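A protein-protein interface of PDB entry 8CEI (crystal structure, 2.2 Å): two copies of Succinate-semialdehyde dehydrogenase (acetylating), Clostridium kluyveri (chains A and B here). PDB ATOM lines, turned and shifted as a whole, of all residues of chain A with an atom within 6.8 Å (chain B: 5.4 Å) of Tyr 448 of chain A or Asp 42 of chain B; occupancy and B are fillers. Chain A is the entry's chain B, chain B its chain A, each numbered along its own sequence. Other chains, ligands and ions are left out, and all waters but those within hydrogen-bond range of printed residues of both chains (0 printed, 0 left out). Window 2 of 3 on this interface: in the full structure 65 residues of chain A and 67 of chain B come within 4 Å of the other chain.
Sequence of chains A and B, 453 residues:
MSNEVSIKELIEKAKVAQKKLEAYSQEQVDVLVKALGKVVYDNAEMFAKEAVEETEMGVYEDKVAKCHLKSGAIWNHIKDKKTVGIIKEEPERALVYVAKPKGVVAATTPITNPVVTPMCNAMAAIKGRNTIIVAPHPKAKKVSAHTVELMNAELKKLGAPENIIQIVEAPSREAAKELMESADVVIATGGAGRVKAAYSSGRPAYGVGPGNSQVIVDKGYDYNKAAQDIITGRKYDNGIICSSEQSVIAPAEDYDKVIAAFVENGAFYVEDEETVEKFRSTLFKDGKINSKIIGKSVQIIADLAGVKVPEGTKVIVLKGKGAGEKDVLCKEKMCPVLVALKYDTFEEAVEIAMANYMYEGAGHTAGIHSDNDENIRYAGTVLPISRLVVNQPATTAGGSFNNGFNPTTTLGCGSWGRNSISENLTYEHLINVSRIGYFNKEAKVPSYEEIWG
Of chain B, only Lys 38, Tyr 41 and Asp 42 come within 4 Å of Tyr 448 of chain A. Of the printed residues of chain B, Trp 452 of chain A touches Gly 37, Lys 38 and Tyr 41. Printed residues of chain A within 4 Å of Gly 37 of chain B: Trp 452 (3.6 Å). Printed residues of chain A within 4 Å of Lys 38 of chain B: Tyr 448 and Trp 452. Printed residues of chain A within 4 Å of Tyr 41 of chain B: Tyr 448 (3.4 Å) and Trp 452 (3.7 Å). Asp 42 of chain B touches one residue of chain A. The nearest printed residue of chain B that does not touch Tyr 448 of chain A is Val 39 of chain B (8.1 Å).
NZ of Lys 38 of chain B lies within salt-bridge range of OD2 of Asp 42 of chain B (3.0 Å).
Among the printed residues, merely in contact across the chains: Tyr 448 of chain A with Tyr 41 of chain B (3.4 Å), Tyr 448 of chain A with Asp 42 of chain B (3.7 Å), Trp 452 of chain A with Gly 37 of chain B (3.6 Å), Trp 452 of chain A with Lys 38 of chain B (3.6 Å) and Trp 452 of chain A with Tyr 41 of chain B (3.7 Å).
NZ of Lys 38 of chain B is in hydrogen-bond range of OH of Tyr 448 of chain A (3.1 Å).
No position is printed for both chains.
Of the 8 printed residues of chain A, 2 touch a printed residue of chain B. Of the 9 printed residues of chain B, 4 touch a printed residue of chain A. Hydrophobic or aromatic side chains of chain B that line the printed part of chain A: Tyr 41. Among the printed residues, 6 pairs touch across the chains.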
ATOM      1  N   PRO A 446      19.422 -18.005  -2.970  1.00  0.00           N
ATOM      2  CA  PRO A 446      18.051 -18.028  -3.490  1.00  0.00           C
ATOM      3  C   PRO A 446      17.970 -18.793  -4.801  1.00  0.00           C
ATOM      4  O   PRO A 446      18.880 -18.737  -5.633  1.00  0.00           O
ATOM      5  CB  PRO A 446      17.718 -16.543  -3.687  1.00  0.00           C
ATOM      6  CG  PRO A 446      18.709 -15.804  -2.833  1.00  0.00           C
ATOM      7  CD  PRO A 446      19.952 -16.636  -2.862  1.00  0.00           C
ATOM      8  N   SER A 447      16.869 -19.518  -4.977  1.00  0.00           N
ATOM      9  CA  SER A 447      16.648 -20.284  -6.193  1.00  0.00           C
ATOM     10  C   SER A 447      16.114 -19.375  -7.298  1.00  0.00           C
ATOM     11  O   SER A 447      15.979 -18.160  -7.131  1.00  0.00           O
ATOM     12  CB  SER A 447      15.693 -21.444  -5.923  1.00  0.00           C
ATOM     13  OG  SER A 447      14.427 -20.973  -5.495  1.00  0.00           O
ATOM     14  N   TYR A 448      15.807 -19.975  -8.451  1.00  0.00           N
ATOM     15  CA  TYR A 448      15.264 -19.203  -9.565  1.00  0.00           C
ATOM     16  C   TYR A 448      13.923 -18.580  -9.199  1.00  0.00           C
ATOM     17  O   TYR A 448      13.639 -17.436  -9.571  1.00  0.00           O
ATOM     18  CB  TYR A 448      15.125 -20.091 -10.802  1.00  0.00           C
ATOM     19  CG  TYR A 448      14.627 -19.360 -12.033  1.00  0.00           C
ATOM     20  CD1 TYR A 448      13.268 -19.278 -12.316  1.00  0.00           C
ATOM     21  CD2 TYR A 448      15.515 -18.759 -12.914  1.00  0.00           C
ATOM     22  CE1 TYR A 448      12.810 -18.613 -13.438  1.00  0.00           C
ATOM     23  CE2 TYR A 448      15.066 -18.092 -14.039  1.00  0.00           C
ATOM     24  CZ  TYR A 448      13.714 -18.022 -14.296  1.00  0.00           C
ATOM     25  OH  TYR A 448      13.266 -17.356 -15.415  1.00  0.00           O
ATOM     26  N   GLU A 449      13.086 -19.321  -8.469  1.00  0.00           N
ATOM     27  CA  GLU A 449      11.792 -18.787  -8.054  1.00  0.00           C
ATOM     28  C   GLU A 449      11.957 -17.637  -7.068  1.00  0.00           C
ATOM     29  O   GLU A 449      11.230 -16.641  -7.141  1.00  0.00           O
ATOM     30  CB  GLU A 449      10.939 -19.902  -7.448  1.00  0.00           C
ATOM     31  CG  GLU A 449       9.733 -19.417  -6.651  1.00  0.00           C
ATOM     32  CD  GLU A 449       8.738 -18.641  -7.495  1.00  0.00           C
ATOM     33  OE1 GLU A 449       8.639 -18.912  -8.711  1.00  0.00           O
ATOM     34  OE2 GLU A 449       8.054 -17.754  -6.939  1.00  0.00           O
ATOM     35  N   GLU A 450      12.914 -17.751  -6.145  1.00  0.00           N
ATOM     36  CA  GLU A 450      13.097 -16.709  -5.140  1.00  0.00           C
ATOM     37  C   GLU A 450      13.614 -15.414  -5.755  1.00  0.00           C
ATOM     38  O   GLU A 450      13.295 -14.326  -5.260  1.00  0.00           O
ATOM     39  CB  GLU A 450      14.051 -17.196  -4.050  1.00  0.00           C
ATOM     40  CG  GLU A 450      13.686 -18.553  -3.471  1.00  0.00           C
ATOM     41  CD  GLU A 450      14.683 -19.031  -2.436  1.00  0.00           C
ATOM     42  OE1 GLU A 450      15.170 -18.196  -1.645  1.00  0.00           O
ATOM     43  OE2 GLU A 450      14.986 -20.243  -2.416  1.00  0.00           O
ATOM     44  N   ILE A 451      14.398 -15.505  -6.827  1.00  0.00           N
ATOM     45  CA  ILE A 451      14.995 -14.312  -7.424  1.00  0.00           C
ATOM     46  C   ILE A 451      14.018 -13.634  -8.376  1.00  0.00           C
ATOM     47  O   ILE A 451      13.705 -12.447  -8.233  1.00  0.00           O
ATOM     48  CB  ILE A 451      16.313 -14.668  -8.136  1.00  0.00           C
ATOM     49  CG1 ILE A 451      17.335 -15.210  -7.137  1.00  0.00           C
ATOM     50  CG2 ILE A 451      16.871 -13.454  -8.860  1.00  0.00           C
ATOM     51  CD1 ILE A 451      18.627 -15.670  -7.777  1.00  0.00           C
ATOM     52  N   TRP A 452      13.521 -14.378  -9.363  1.00  0.00           N
ATOM     53  CA  TRP A 452      12.722 -13.810 -10.439  1.00  0.00           C
ATOM     54  C   TRP A 452      11.223 -13.994 -10.245  1.00  0.00           C
ATOM     55  O   TRP A 452      10.449 -13.631 -11.136  1.00  0.00           O
ATOM     56  CB  TRP A 452      13.146 -14.419 -11.779  1.00  0.00           C
ATOM     57  CG  TRP A 452      14.625 -14.373 -12.001  1.00  0.00           C
ATOM     58  CD1 TRP A 452      15.502 -15.416 -11.910  1.00  0.00           C
ATOM     59  CD2 TRP A 452      15.406 -13.220 -12.338  1.00  0.00           C
ATOM     60  NE1 TRP A 452      16.779 -14.984 -12.176  1.00  0.00           N
ATOM     61  CE2 TRP A 452      16.747 -13.640 -12.441  1.00  0.00           C
ATOM     62  CE3 TRP A 452      15.100 -11.875 -12.563  1.00  0.00           C
ATOM     63  CZ2 TRP A 452      17.780 -12.764 -12.762  1.00  0.00           C
ATOM     64  CZ3 TRP A 452      16.127 -11.007 -12.881  1.00  0.00           C
ATOM     65  CH2 TRP A 452      17.451 -11.454 -12.978  1.00  0.00           C
ATOM     66  N   GLY A 453      10.793 -14.543  -9.114  1.00  0.00           N
ATOM     67  CA  GLY A 453       9.377 -14.734  -8.860  1.00  0.00           C
ATOM     68  C   GLY A 453       8.672 -13.452  -8.463  1.00  0.00           C
ATOM     69  O   GLY A 453       9.315 -12.485  -8.055  1.00  0.00           O
ATOM     70  N   GLY B  37      17.880  -7.570 -16.237  1.00  0.00           N
ATOM     71  CA  GLY B  37      18.696  -8.672 -15.766  1.00  0.00           C
ATOM     72  C   GLY B  37      18.158 -10.028 -16.175  1.00  0.00           C
ATOM     73  O   GLY B  37      18.932 -10.956 -16.428  1.00  0.00           O
ATOM     74  N   LYS B  38      16.832 -10.161 -16.259  1.00  0.00           N
ATOM     75  CA  LYS B  38      16.242 -11.457 -16.571  1.00  0.00           C
ATOM     76  C   LYS B  38      16.525 -11.879 -18.008  1.00  0.00           C
ATOM     77  O   LYS B  38      16.663 -13.076 -18.282  1.00  0.00           O
ATOM     78  CB  LYS B  38      14.736 -11.424 -16.311  1.00  0.00           C
ATOM     79  CG  LYS B  38      14.090 -12.800 -16.263  1.00  0.00           C
ATOM     80  CD  LYS B  38      12.623 -12.717 -15.873  1.00  0.00           C
ATOM     81  CE  LYS B  38      12.019 -14.104 -15.715  1.00  0.00           C
ATOM     82  NZ  LYS B  38      12.133 -14.909 -16.963  1.00  0.00           N
ATOM     83  N   VAL B  39      16.623 -10.922 -18.935  1.00  0.00           N
ATOM     84  CA  VAL B  39      16.895 -11.281 -20.324  1.00  0.00           C
ATOM     85  C   VAL B  39      18.343 -11.729 -20.486  1.00  0.00           C
ATOM     86  O   VAL B  39      18.654 -12.535 -21.372  1.00  0.00           O
ATOM     87  CB  VAL B  39      16.545 -10.110 -21.265  1.00  0.00           C
ATOM     88  CG1 VAL B  39      17.556  -8.984 -21.139  1.00  0.00           C
ATOM     89  CG2 VAL B  39      16.447 -10.594 -22.706  1.00  0.00           C
ATOM     90  N   VAL B  40      19.247 -11.231 -19.640  1.00  0.00           N
ATOM     91  CA  VAL B  40      20.617 -11.730 -19.649  1.00  0.00           C
ATOM     92  C   VAL B  40      20.674 -13.119 -19.028  1.00  0.00           C
ATOM     93  O   VAL B  40      21.407 -13.998 -19.500  1.00  0.00           O
ATOM     94  CB  VAL B  40      21.550 -10.739 -18.929  1.00  0.00           C
ATOM     95  CG1 VAL B  40      22.918 -11.360 -18.690  1.00  0.00           C
ATOM     96  CG2 VAL B  40      21.680  -9.464 -19.739  1.00  0.00           C
ATOM     97  N   TYR B  41      19.891 -13.345 -17.969  1.00  0.00           N
ATOM     98  CA  TYR B  41      19.806 -14.678 -17.382  1.00  0.00           C
ATOM     99  C   TYR B  41      19.219 -15.676 -18.373  1.00  0.00           C
ATOM    100  O   TYR B  41      19.732 -16.791 -18.520  1.00  0.00           O
ATOM    101  CB  TYR B  41      18.966 -14.634 -16.101  1.00  0.00           C
ATOM    102  CG  TYR B  41      19.039 -15.897 -15.265  1.00  0.00           C
ATOM    103  CD1 TYR B  41      18.335 -17.041 -15.629  1.00  0.00           C
ATOM    104  CD2 TYR B  41      19.803 -15.943 -14.108  1.00  0.00           C
ATOM    105  CE1 TYR B  41      18.401 -18.195 -14.870  1.00  0.00           C
ATOM    106  CE2 TYR B  41      19.873 -17.092 -13.340  1.00  0.00           C
ATOM    107  CZ  TYR B  41      19.169 -18.215 -13.726  1.00  0.00           C
ATOM    108  OH  TYR B  41      19.235 -19.362 -12.966  1.00  0.00           O
ATOM    109  N   ASP B  42      18.144 -15.289 -19.066  1.00  0.00           N
ATOM    110  CA  ASP B  42      17.459 -16.206 -19.968  1.00  0.00           C
ATOM    111  C   ASP B  42      18.259 -16.500 -21.232  1.00  0.00           C
ATOM    112  O   ASP B  42      18.034 -17.538 -21.861  1.00  0.00           O
ATOM    113  CB  ASP B  42      16.086 -15.646 -20.345  1.00  0.00           C
ATOM    114  CG  ASP B  42      15.130 -15.601 -19.168  1.00  0.00           C
ATOM    115  OD1 ASP B  42      15.487 -16.117 -18.089  1.00  0.00           O
ATOM    116  OD2 ASP B  42      14.021 -15.047 -19.322  1.00  0.00           O
ATOM    117  N   ASN B  43      19.176 -15.615 -21.621  1.00  0.00           N
ATOM    118  CA  ASN B  43      19.991 -15.801 -22.815  1.00  0.00           C
ATOM    119  C   ASN B  43      21.467 -15.991 -22.471  1.00  0.00           C
ATOM    120  O   ASN B  43      22.345 -15.655 -23.271  1.00  0.00           O
ATOM    121  CB  ASN B  43      19.816 -14.625 -23.773  1.00  0.00           C
ATOM    122  CG  ASN B  43      18.387 -14.472 -24.250  1.00  0.00           C
ATOM    123  OD1 ASN B  43      17.986 -15.078 -25.243  1.00  0.00           O
ATOM    124  ND2 ASN B  43      17.610 -13.659 -23.544  1.00  0.00           N
ATOM    125  N   ALA B  44      21.746 -16.534 -21.284  1.00  0.00           N
ATOM    126  CA  ALA B  44      23.126 -16.678 -20.830  1.00  0.00           C
ATOM    127  C   ALA B  44      23.937 -17.557 -21.773  1.00  0.00           C
ATOM    128  O   ALA B  44      25.109 -17.273 -22.044  1.00  0.00           O
ATOM    129  CB  ALA B  44      23.149 -17.252 -19.415  1.00  0.00           C
ATOM    130  N   GLU B  45      23.326 -18.627 -22.289  1.00  0.00           N
ATOM    131  CA  GLU B  45      24.060 -19.566 -23.131  1.00  0.00           C
ATOM    132  C   GLU B  45      24.442 -18.937 -24.466  1.00  0.00           C
ATOM    133  O   GLU B  45      25.544 -19.173 -24.975  1.00  0.00           O
ATOM    134  CB  GLU B  45      23.230 -20.833 -23.352  1.00  0.00           C
ATOM    135  CG  GLU B  45      23.026 -21.680 -22.101  1.00  0.00           C
ATOM    136  CD  GLU B  45      21.981 -21.111 -21.158  1.00  0.00           C
ATOM    137  OE1 GLU B  45      21.198 -20.237 -21.587  1.00  0.00           O
ATOM    138  OE2 GLU B  45      21.944 -21.539 -19.985  1.00  0.00           O
